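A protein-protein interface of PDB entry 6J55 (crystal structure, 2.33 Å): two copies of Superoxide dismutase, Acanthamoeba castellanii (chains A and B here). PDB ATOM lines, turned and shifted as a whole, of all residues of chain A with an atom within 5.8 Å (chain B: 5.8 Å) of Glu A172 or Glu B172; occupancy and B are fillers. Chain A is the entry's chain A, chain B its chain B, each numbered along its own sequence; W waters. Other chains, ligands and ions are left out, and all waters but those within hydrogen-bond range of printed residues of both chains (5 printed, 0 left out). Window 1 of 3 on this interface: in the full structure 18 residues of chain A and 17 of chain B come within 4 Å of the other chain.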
ATOM      1  N   HIS A  39     -22.153   2.488  10.970  1.00  0.00           N
ATOM      2  CA  HIS A  39     -22.791   1.559  10.040  1.00  0.00           C
ATOM      3  C   HIS A  39     -23.682   2.285   9.028  1.00  0.00           C
ATOM      4  O   HIS A  39     -23.540   2.094   7.820  1.00  0.00           O
ATOM      5  CB  HIS A  39     -23.599   0.528  10.832  1.00  0.00           C
ATOM      6  CG  HIS A  39     -22.756  -0.298  11.760  1.00  0.00           C
ATOM      7  ND1 HIS A  39     -22.009  -1.371  11.328  1.00  0.00           N
ATOM      8  CD2 HIS A  39     -22.488  -0.161  13.080  1.00  0.00           C
ATOM      9  CE1 HIS A  39     -21.333  -1.871  12.343  1.00  0.00           C
ATOM     10  NE2 HIS A  39     -21.593  -1.147  13.411  1.00  0.00           N
ATOM     11  N   GLY A 133     -28.029 -15.266  13.890  1.00  0.00           N
ATOM     12  CA  GLY A 133     -27.110 -14.431  13.128  1.00  0.00           C
ATOM     13  C   GLY A 133     -27.585 -12.989  13.069  1.00  0.00           C
ATOM     14  O   GLY A 133     -28.276 -12.511  13.962  1.00  0.00           O
ATOM     15  N   SER A 134     -27.189 -12.294  12.001  1.00  0.00           N
ATOM     16  CA  SER A 134     -27.577 -10.906  11.756  1.00  0.00           C
ATOM     17  C   SER A 134     -28.924 -10.833  11.051  1.00  0.00           C
ATOM     18  O   SER A 134     -29.210 -11.617  10.138  1.00  0.00           O
ATOM     19  CB  SER A 134     -26.542 -10.190  10.886  1.00  0.00           C
ATOM     20  OG  SER A 134     -25.246 -10.326  11.431  1.00  0.00           O
ATOM     21  N   VAL A 170     -31.359  -6.869  15.108  1.00  0.00           N
ATOM     22  CA  VAL A 170     -30.633  -7.808  15.954  1.00  0.00           C
ATOM     23  C   VAL A 170     -29.285  -8.191  15.382  1.00  0.00           C
ATOM     24  O   VAL A 170     -28.659  -9.125  15.866  1.00  0.00           O
ATOM     25  CB  VAL A 170     -31.448  -9.076  16.321  1.00  0.00           C
ATOM     26  CG1 VAL A 170     -32.802  -8.708  16.910  1.00  0.00           C
ATOM     27  CG2 VAL A 170     -31.633  -9.983  15.073  1.00  0.00           C
ATOM     28  N   TRP A 171     -28.809  -7.478  14.369  1.00  0.00           N
ATOM     29  CA  TRP A 171     -27.376  -7.470  14.140  1.00  0.00           C
ATOM     30  C   TRP A 171     -26.693  -7.157  15.474  1.00  0.00           C
ATOM     31  O   TRP A 171     -27.161  -6.312  16.240  1.00  0.00           O
ATOM     32  CB  TRP A 171     -27.002  -6.402  13.100  1.00  0.00           C
ATOM     33  CG  TRP A 171     -27.278  -6.719  11.673  1.00  0.00           C
ATOM     34  CD1 TRP A 171     -28.509  -6.951  11.086  1.00  0.00           C
ATOM     35  CD2 TRP A 171     -26.318  -6.791  10.621  1.00  0.00           C
ATOM     36  NE1 TRP A 171     -28.352  -7.176   9.740  1.00  0.00           N
ATOM     37  CE2 TRP A 171     -27.020  -7.077   9.427  1.00  0.00           C
ATOM     38  CE3 TRP A 171     -24.931  -6.649  10.570  1.00  0.00           C
ATOM     39  CZ2 TRP A 171     -26.379  -7.233   8.207  1.00  0.00           C
ATOM     40  CZ3 TRP A 171     -24.304  -6.790   9.360  1.00  0.00           C
ATOM     41  CH2 TRP A 171     -25.030  -7.085   8.188  1.00  0.00           C
ATOM     42  N   GLU A 172     -25.593  -7.848  15.763  1.00  0.00           N
ATOM     43  CA  GLU A 172     -24.987  -7.693  17.081  1.00  0.00           C
ATOM     44  C   GLU A 172     -24.507  -6.259  17.343  1.00  0.00           C
ATOM     45  O   GLU A 172     -24.477  -5.830  18.505  1.00  0.00           O
ATOM     46  CB  GLU A 172     -23.832  -8.676  17.246  1.00  0.00           C
ATOM     47  CG  GLU A 172     -24.335 -10.061  17.664  1.00  0.00           C
ATOM     48  CD  GLU A 172     -23.258 -11.118  17.640  1.00  0.00           C
ATOM     49  OE1 GLU A 172     -22.361 -11.039  16.766  1.00  0.00           O
ATOM     50  OE2 GLU A 172     -23.318 -12.033  18.500  1.00  0.00           O
ATOM     51  N   HIS A 173     -24.145  -5.500  16.292  1.00  0.00           N
ATOM     52  CA  HIS A 173     -23.692  -4.131  16.532  1.00  0.00           C
ATOM     53  C   HIS A 173     -24.786  -3.251  17.110  1.00  0.00           C
ATOM     54  O   HIS A 173     -24.477  -2.224  17.732  1.00  0.00           O
ATOM     55  CB  HIS A 173     -23.105  -3.492  15.261  1.00  0.00           C
ATOM     56  CG  HIS A 173     -24.056  -3.360  14.112  1.00  0.00           C
ATOM     57  ND1 HIS A 173     -23.781  -3.886  12.866  1.00  0.00           N
ATOM     58  CD2 HIS A 173     -25.265  -2.755  14.006  1.00  0.00           C
ATOM     59  CE1 HIS A 173     -24.768  -3.592  12.037  1.00  0.00           C
ATOM     60  NE2 HIS A 173     -25.684  -2.914  12.706  1.00  0.00           N
ATOM     61  N   ALA A 174     -26.054  -3.654  16.968  1.00  0.00           N
ATOM     62  CA  ALA A 174     -27.150  -2.874  17.533  1.00  0.00           C
ATOM     63  C   ALA A 174     -27.175  -2.907  19.061  1.00  0.00           C
ATOM     64  O   ALA A 174     -27.783  -2.027  19.691  1.00  0.00           O
ATOM     65  CB  ALA A 174     -28.480  -3.384  16.975  1.00  0.00           C
ATOM     66  N   TYR A 175     -26.531  -3.892  19.677  1.00  0.00           N
ATOM     67  CA  TYR A 175     -26.652  -4.047  21.120  1.00  0.00           C
ATOM     68  C   TYR A 175     -25.397  -4.510  21.834  1.00  0.00           C
ATOM     69  O   TYR A 175     -25.402  -4.513  23.064  1.00  0.00           O
ATOM     70  CB  TYR A 175     -27.777  -5.032  21.459  1.00  0.00           C
ATOM     71  CG  TYR A 175     -27.613  -6.440  20.885  1.00  0.00           C
ATOM     72  CD1 TYR A 175     -26.863  -7.416  21.555  1.00  0.00           C
ATOM     73  CD2 TYR A 175     -28.274  -6.817  19.704  1.00  0.00           C
ATOM     74  CE1 TYR A 175     -26.741  -8.707  21.055  1.00  0.00           C
ATOM     75  CE2 TYR A 175     -28.159  -8.126  19.185  1.00  0.00           C
ATOM     76  CZ  TYR A 175     -27.388  -9.064  19.875  1.00  0.00           C
ATOM     77  OH  TYR A 175     -27.265 -10.354  19.391  1.00  0.00           O
ATOM     78  N   TYR A 176     -24.319  -4.868  21.140  1.00  0.00           N
ATOM     79  CA  TYR A 176     -23.229  -5.551  21.834  1.00  0.00           C
ATOM     80  C   TYR A 176     -22.499  -4.625  22.814  1.00  0.00           C
ATOM     81  O   TYR A 176     -22.011  -5.094  23.848  1.00  0.00           O
ATOM     82  CB  TYR A 176     -22.249  -6.160  20.828  1.00  0.00           C
ATOM     83  CG  TYR A 176     -21.661  -7.457  21.335  1.00  0.00           C
ATOM     84  CD1 TYR A 176     -22.394  -8.627  21.298  1.00  0.00           C
ATOM     85  CD2 TYR A 176     -20.393  -7.498  21.912  1.00  0.00           C
ATOM     86  CE1 TYR A 176     -21.875  -9.804  21.784  1.00  0.00           C
ATOM     87  CE2 TYR A 176     -19.864  -8.682  22.400  1.00  0.00           C
ATOM     88  CZ  TYR A 176     -20.613  -9.828  22.335  1.00  0.00           C
ATOM     89  OH  TYR A 176     -20.107 -11.018  22.810  1.00  0.00           O
ATOM     90  N   LEU A 177     -22.399  -3.319  22.513  1.00  0.00           N
ATOM     91  CA  LEU A 177     -21.683  -2.422  23.413  1.00  0.00           C
ATOM     92  C   LEU A 177     -22.400  -2.282  24.740  1.00  0.00           C
ATOM     93  O   LEU A 177     -21.748  -2.087  25.776  1.00  0.00           O
ATOM     94  CB  LEU A 177     -21.492  -1.032  22.801  1.00  0.00           C
ATOM     95  CG  LEU A 177     -20.626  -0.909  21.548  1.00  0.00           C
ATOM     96  CD1 LEU A 177     -20.666   0.518  21.037  1.00  0.00           C
ATOM     97  CD2 LEU A 177     -19.198  -1.341  21.806  1.00  0.00           C
ATOM     98  N   ARG A 183     -28.809 -10.626  24.205  1.00  0.00           N
ATOM     99  CA  ARG A 183     -29.857 -10.092  23.340  1.00  0.00           C
ATOM    100  C   ARG A 183     -31.217 -10.052  24.011  1.00  0.00           C
ATOM    101  O   ARG A 183     -31.934  -9.051  23.813  1.00  0.00           O
ATOM    102  CB  ARG A 183     -29.957 -10.909  22.045  1.00  0.00           C
ATOM    103  CG  ARG A 183     -30.841 -10.254  20.956  1.00  0.00           C
ATOM    104  CD  ARG A 183     -31.162 -11.231  19.847  1.00  0.00           C
ATOM    105  NE  ARG A 183     -30.019 -11.374  18.973  1.00  0.00           N
ATOM    106  CZ  ARG A 183     -30.035 -12.088  17.854  1.00  0.00           C
ATOM    107  NH1 ARG A 183     -31.146 -12.718  17.493  1.00  0.00           N
ATOM    108  NH2 ARG A 183     -28.955 -12.169  17.093  1.00  0.00           N
ATOM    109  N   HIS B  39     -20.445 -16.736  24.397  1.00  0.00           N
ATOM    110  CA  HIS B  39     -20.923 -17.389  23.179  1.00  0.00           C
ATOM    111  C   HIS B  39     -20.543 -18.881  23.130  1.00  0.00           C
ATOM    112  O   HIS B  39     -21.397 -19.735  22.868  1.00  0.00           O
ATOM    113  CB  HIS B  39     -20.426 -16.627  21.938  1.00  0.00           C
ATOM    114  CG  HIS B  39     -20.942 -15.218  21.847  1.00  0.00           C
ATOM    115  ND1 HIS B  39     -22.220 -14.920  21.430  1.00  0.00           N
ATOM    116  CD2 HIS B  39     -20.366 -14.031  22.152  1.00  0.00           C
ATOM    117  CE1 HIS B  39     -22.407 -13.612  21.475  1.00  0.00           C
ATOM    118  NE2 HIS B  39     -21.295 -13.052  21.900  1.00  0.00           N
ATOM    119  N   GLY B 133     -22.640  -9.720   6.868  1.00  0.00           N
ATOM    120  CA  GLY B 133     -23.340 -10.274   8.025  1.00  0.00           C
ATOM    121  C   GLY B 133     -22.418 -11.078   8.938  1.00  0.00           C
ATOM    122  O   GLY B 133     -21.213 -10.841   8.996  1.00  0.00           O
ATOM    123  N   SER B 134     -23.003 -12.046   9.660  1.00  0.00           N
ATOM    124  CA  SER B 134     -22.235 -12.937  10.535  1.00  0.00           C
ATOM    125  C   SER B 134     -21.661 -14.106   9.740  1.00  0.00           C
ATOM    126  O   SER B 134     -22.312 -14.651   8.847  1.00  0.00           O
ATOM    127  CB  SER B 134     -23.117 -13.503  11.660  1.00  0.00           C
ATOM    128  OG  SER B 134     -23.822 -12.512  12.389  1.00  0.00           O
ATOM    129  N   VAL B 170     -15.863 -13.566  11.843  1.00  0.00           N
ATOM    130  CA  VAL B 170     -16.306 -12.218  11.517  1.00  0.00           C
ATOM    131  C   VAL B 170     -17.734 -11.936  11.969  1.00  0.00           C
ATOM    132  O   VAL B 170     -18.309 -10.918  11.586  1.00  0.00           O
ATOM    133  CB  VAL B 170     -16.132 -11.882  10.016  1.00  0.00           C
ATOM    134  CG1 VAL B 170     -14.748 -12.300   9.523  1.00  0.00           C
ATOM    135  CG2 VAL B 170     -17.210 -12.568   9.181  1.00  0.00           C
ATOM    136  N   TRP B 171     -18.320 -12.809  12.791  1.00  0.00           N
ATOM    137  CA  TRP B 171     -19.438 -12.376  13.610  1.00  0.00           C
ATOM    138  C   TRP B 171     -19.013 -11.119  14.374  1.00  0.00           C
ATOM    139  O   TRP B 171     -17.856 -10.997  14.815  1.00  0.00           O
ATOM    140  CB  TRP B 171     -19.868 -13.473  14.597  1.00  0.00           C
ATOM    141  CG  TRP B 171     -20.713 -14.645  14.077  1.00  0.00           C
ATOM    142  CD1 TRP B 171     -20.357 -15.586  13.149  1.00  0.00           C
ATOM    143  CD2 TRP B 171     -22.029 -15.013  14.530  1.00  0.00           C
ATOM    144  NE1 TRP B 171     -21.374 -16.508  12.993  1.00  0.00           N
ATOM    145  CE2 TRP B 171     -22.407 -16.178  13.827  1.00  0.00           C
ATOM    146  CE3 TRP B 171     -22.920 -14.467  15.464  1.00  0.00           C
ATOM    147  CZ2 TRP B 171     -23.645 -16.788  14.008  1.00  0.00           C
ATOM    148  CZ3 TRP B 171     -24.137 -15.070  15.651  1.00  0.00           C
ATOM    149  CH2 TRP B 171     -24.496 -16.231  14.927  1.00  0.00           C
ATOM    150  N   GLU B 172     -19.947 -10.165  14.500  1.00  0.00           N
ATOM    151  CA  GLU B 172     -19.577  -8.885  15.085  1.00  0.00           C
ATOM    152  C   GLU B 172     -19.147  -9.051  16.541  1.00  0.00           C
ATOM    153  O   GLU B 172     -18.252  -8.336  17.001  1.00  0.00           O
ATOM    154  CB  GLU B 172     -20.729  -7.883  14.935  1.00  0.00           C
ATOM    155  CG  GLU B 172     -20.760  -7.210  13.543  1.00  0.00           C
ATOM    156  CD  GLU B 172     -21.991  -6.326  13.297  1.00  0.00           C
ATOM    157  OE1 GLU B 172     -21.846  -5.326  12.546  1.00  0.00           O
ATOM    158  OE2 GLU B 172     -23.098  -6.632  13.822  1.00  0.00           O
ATOM    159  N   HIS B 173     -19.688 -10.051  17.250  1.00  0.00           N
ATOM    160  CA  HIS B 173     -19.262 -10.230  18.629  1.00  0.00           C
ATOM    161  C   HIS B 173     -17.787 -10.594  18.729  1.00  0.00           C
ATOM    162  O   HIS B 173     -17.213 -10.460  19.808  1.00  0.00           O
ATOM    163  CB  HIS B 173     -20.125 -11.265  19.390  1.00  0.00           C
ATOM    164  CG  HIS B 173     -20.077 -12.652  18.839  1.00  0.00           C
ATOM    165  ND1 HIS B 173     -21.217 -13.335  18.475  1.00  0.00           N
ATOM    166  CD2 HIS B 173     -19.037 -13.475  18.562  1.00  0.00           C
ATOM    167  CE1 HIS B 173     -20.879 -14.524  18.004  1.00  0.00           C
ATOM    168  NE2 HIS B 173     -19.562 -14.635  18.049  1.00  0.00           N
ATOM    169  N   ALA B 174     -17.156 -11.043  17.643  1.00  0.00           N
ATOM    170  CA  ALA B 174     -15.736 -11.375  17.718  1.00  0.00           C
ATOM    171  C   ALA B 174     -14.849 -10.149  17.888  1.00  0.00           C
ATOM    172  O   ALA B 174     -13.703 -10.288  18.346  1.00  0.00           O
ATOM    173  CB  ALA B 174     -15.274 -12.109  16.468  1.00  0.00           C
ATOM    174  N   TYR B 175     -15.346  -8.962  17.517  1.00  0.00           N
ATOM    175  CA  TYR B 175     -14.500  -7.786  17.453  1.00  0.00           C
ATOM    176  C   TYR B 175     -15.155  -6.484  17.884  1.00  0.00           C
ATOM    177  O   TYR B 175     -14.439  -5.483  17.978  1.00  0.00           O
ATOM    178  CB  TYR B 175     -13.961  -7.598  16.023  1.00  0.00           C
ATOM    179  CG  TYR B 175     -15.011  -7.421  14.922  1.00  0.00           C
ATOM    180  CD1 TYR B 175     -15.565  -6.175  14.641  1.00  0.00           C
ATOM    181  CD2 TYR B 175     -15.398  -8.501  14.129  1.00  0.00           C
ATOM    182  CE1 TYR B 175     -16.519  -6.017  13.623  1.00  0.00           C
ATOM    183  CE2 TYR B 175     -16.334  -8.367  13.131  1.00  0.00           C
ATOM    184  CZ  TYR B 175     -16.899  -7.120  12.866  1.00  0.00           C
ATOM    185  OH  TYR B 175     -17.826  -7.007  11.838  1.00  0.00           O
ATOM    186  N   TYR B 176     -16.462  -6.445  18.172  1.00  0.00           N
ATOM    187  CA  TYR B 176     -17.114  -5.146  18.297  1.00  0.00           C
ATOM    188  C   TYR B 176     -16.647  -4.389  19.541  1.00  0.00           C
ATOM    189  O   TYR B 176     -16.571  -3.152  19.513  1.00  0.00           O
ATOM    190  CB  TYR B 176     -18.633  -5.293  18.303  1.00  0.00           C
ATOM    191  CG  TYR B 176     -19.302  -4.117  17.648  1.00  0.00           C
ATOM    192  CD1 TYR B 176     -19.325  -4.001  16.258  1.00  0.00           C
ATOM    193  CD2 TYR B 176     -19.860  -3.079  18.412  1.00  0.00           C
ATOM    194  CE1 TYR B 176     -19.896  -2.909  15.646  1.00  0.00           C
ATOM    195  CE2 TYR B 176     -20.438  -1.976  17.807  1.00  0.00           C
ATOM    196  CZ  TYR B 176     -20.450  -1.894  16.421  1.00  0.00           C
ATOM    197  OH  TYR B 176     -21.024  -0.815  15.789  1.00  0.00           O
ATOM    198  N   LEU B 177     -16.357  -5.104  20.645  1.00  0.00           N
ATOM    199  CA  LEU B 177     -15.921  -4.431  21.868  1.00  0.00           C
ATOM    200  C   LEU B 177     -14.557  -3.776  21.691  1.00  0.00           C
ATOM    201  O   LEU B 177     -14.292  -2.734  22.296  1.00  0.00           O
ATOM    202  CB  LEU B 177     -15.887  -5.399  23.042  1.00  0.00           C
ATOM    203  CG  LEU B 177     -17.215  -5.981  23.525  1.00  0.00           C
ATOM    204  CD1 LEU B 177     -16.939  -7.054  24.565  1.00  0.00           C
ATOM    205  CD2 LEU B 177     -18.076  -4.889  24.122  1.00  0.00           C
ATOM    206  N   ARG B 183     -14.119  -3.468  11.097  1.00  0.00           N
ATOM    207  CA  ARG B 183     -13.711  -4.832  10.779  1.00  0.00           C
ATOM    208  C   ARG B 183     -12.379  -4.910  10.032  1.00  0.00           C
ATOM    209  O   ARG B 183     -11.593  -5.818  10.334  1.00  0.00           O
ATOM    210  CB  ARG B 183     -14.821  -5.550   9.991  1.00  0.00           C
ATOM    211  CG  ARG B 183     -14.587  -7.080   9.830  1.00  0.00           C
ATOM    212  CD  ARG B 183     -15.489  -7.744   8.777  1.00  0.00           C
ATOM    213  NE  ARG B 183     -16.833  -7.965   9.315  1.00  0.00           N
ATOM    214  CZ  ARG B 183     -17.801  -8.613   8.671  1.00  0.00           C
ATOM    215  NH1 ARG B 183     -17.587  -9.117   7.468  1.00  0.00           N
ATOM    216  NH2 ARG B 183     -18.982  -8.757   9.241  1.00  0.00           N
HETATM  217  O   HOH W   1     -17.682 -11.732  22.441  1.00  0.00           O
HETATM  218  O   HOH W   2     -25.738 -13.305   9.510  1.00  0.00           O
HETATM  219  O   HOH W   3     -23.281   0.097  16.573  1.00  0.00           O
HETATM  220  O   HOH W   4     -22.656 -10.868  14.160  1.00  0.00           O
HETATM  221  O   HOH W   5     -24.514  -9.007  13.696  1.00  0.00           O
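Among the printed residues, merely in contact across the chains: His A173 with Tyr B176, Tyr A176 with His B173, Glu A172 with His B39, His A39 with Glu B172, Trp A171 with Gly B133, Gly A133 with Trp B171, Glu A172 with Trp B171, Trp A171 with Glu B172, Ser A134 with Gly B133, Gly A133 with Ser B134, Leu A177 with Tyr B176 and Tyr A176 with Leu B177.
Hydrophobic or aromatic side chains of chain B within 4 Å of the printed part of chain A: His B39, Trp B171, His B173, Tyr B176 and Leu B177. Among the printed residues, 18 pairs touch across the chains.
A ring nitrogen (NE2) of His A39 is in hydrogen-bond range of the side-chain hydroxyl (OH) of Tyr B176 (2.5 Å). OG of Ser A134 is in hydrogen-bond range of OG of Ser B134 (2.8 Å). The backbone NH of Glu A172 sits at hydrogen-bond distance from the side-chain carboxylate of Glu B172 (3.4 Å). OE2 of Glu A172 sits at hydrogen-bond distance from ND1 of His B173, at 2.5 Å. A ring nitrogen (ND1) of His A173 is in hydrogen-bond range of the side-chain carboxylate (OE1) of Glu B172. OH of Tyr A176 sits at hydrogen-bond distance from NE2 of His B39, 2.5 Å away.
Water W1 bridges OH of Tyr A176 (2.6 Å) and O of His B173 (3.0 Å). Water W3 lies within hydrogen-bond range of the side-chain hydroxyl of Tyr B176 and the backbone carbonyl oxygen of His A173. Water W5 lies within hydrogen-bond range of N of Glu A172, OG of Ser A134 and OE2 of Glu B172. Water W4 lies within hydrogen-bond range of OE1 of Glu A172 (2.6 Å), OG of Ser B134 (2.7 Å) and N of Glu B172 (2.8 Å). Water W2 bridges the backbone NH (N) of Ser B134 and the backbone NH (N) of Ser A134.
Printed residues of chain B within 4 Å of Glu A172: His B39 (3.5 Å), Trp B171 (3.7 Å), Glu B172 (3.4 Å) and His B173 (2.5 Å). Glu B172 touches just these residues of chain A: His A39, Trp A171, Glu A172 and His A173. Of the printed residues of chain A, Leu B177 touches Tyr A176. Of the printed residues of chain A, Trp B171 touches Gly A133 and Glu A172. Printed residues of chain A within 4 Å of Gly B133: Ser A134 and Trp A171. Printed residues of chain A within 4 Å of Ser B134: Gly A133 and Ser A134. Ala A174 touches none of the printed residues of chain B. The nearest residue of chain B that does not touch Glu A172 is Ser B134 (4.8 Å). The nearest residue of chain A that does not touch Glu B172 is Ser A134 (4.9 Å).
ND1 of His A39 lies close to ND1 of His A173 (3.4 Å). NH2 of Arg A183 sits at hydrogen-bond distance from O of Gly A133, at 3.2 Å. A ring nitrogen (NE2) of His B39 lies close to a ring nitrogen (ND1) of His B173, at 3.4 Å. The guanidinium group (NH2) of Arg B183 sits at hydrogen-bond distance from the backbone carbonyl oxygen (O) of Gly B133 (3.1 Å).
His A39 touches Glu B172, and with the chains exchanged Glu A172 touches His B39. Gly A133 touches Ser B134, and with the chains exchanged Ser A134 touches Gly B133. Glu A172 touches its own counterpart, Glu B172. His A173 touches Tyr B176, and with the chains exchanged Tyr A176 touches His B173. Of the 18 pairs that touch across the chains among the printed residues, 18 have their exchanged pair printed and touching as well.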
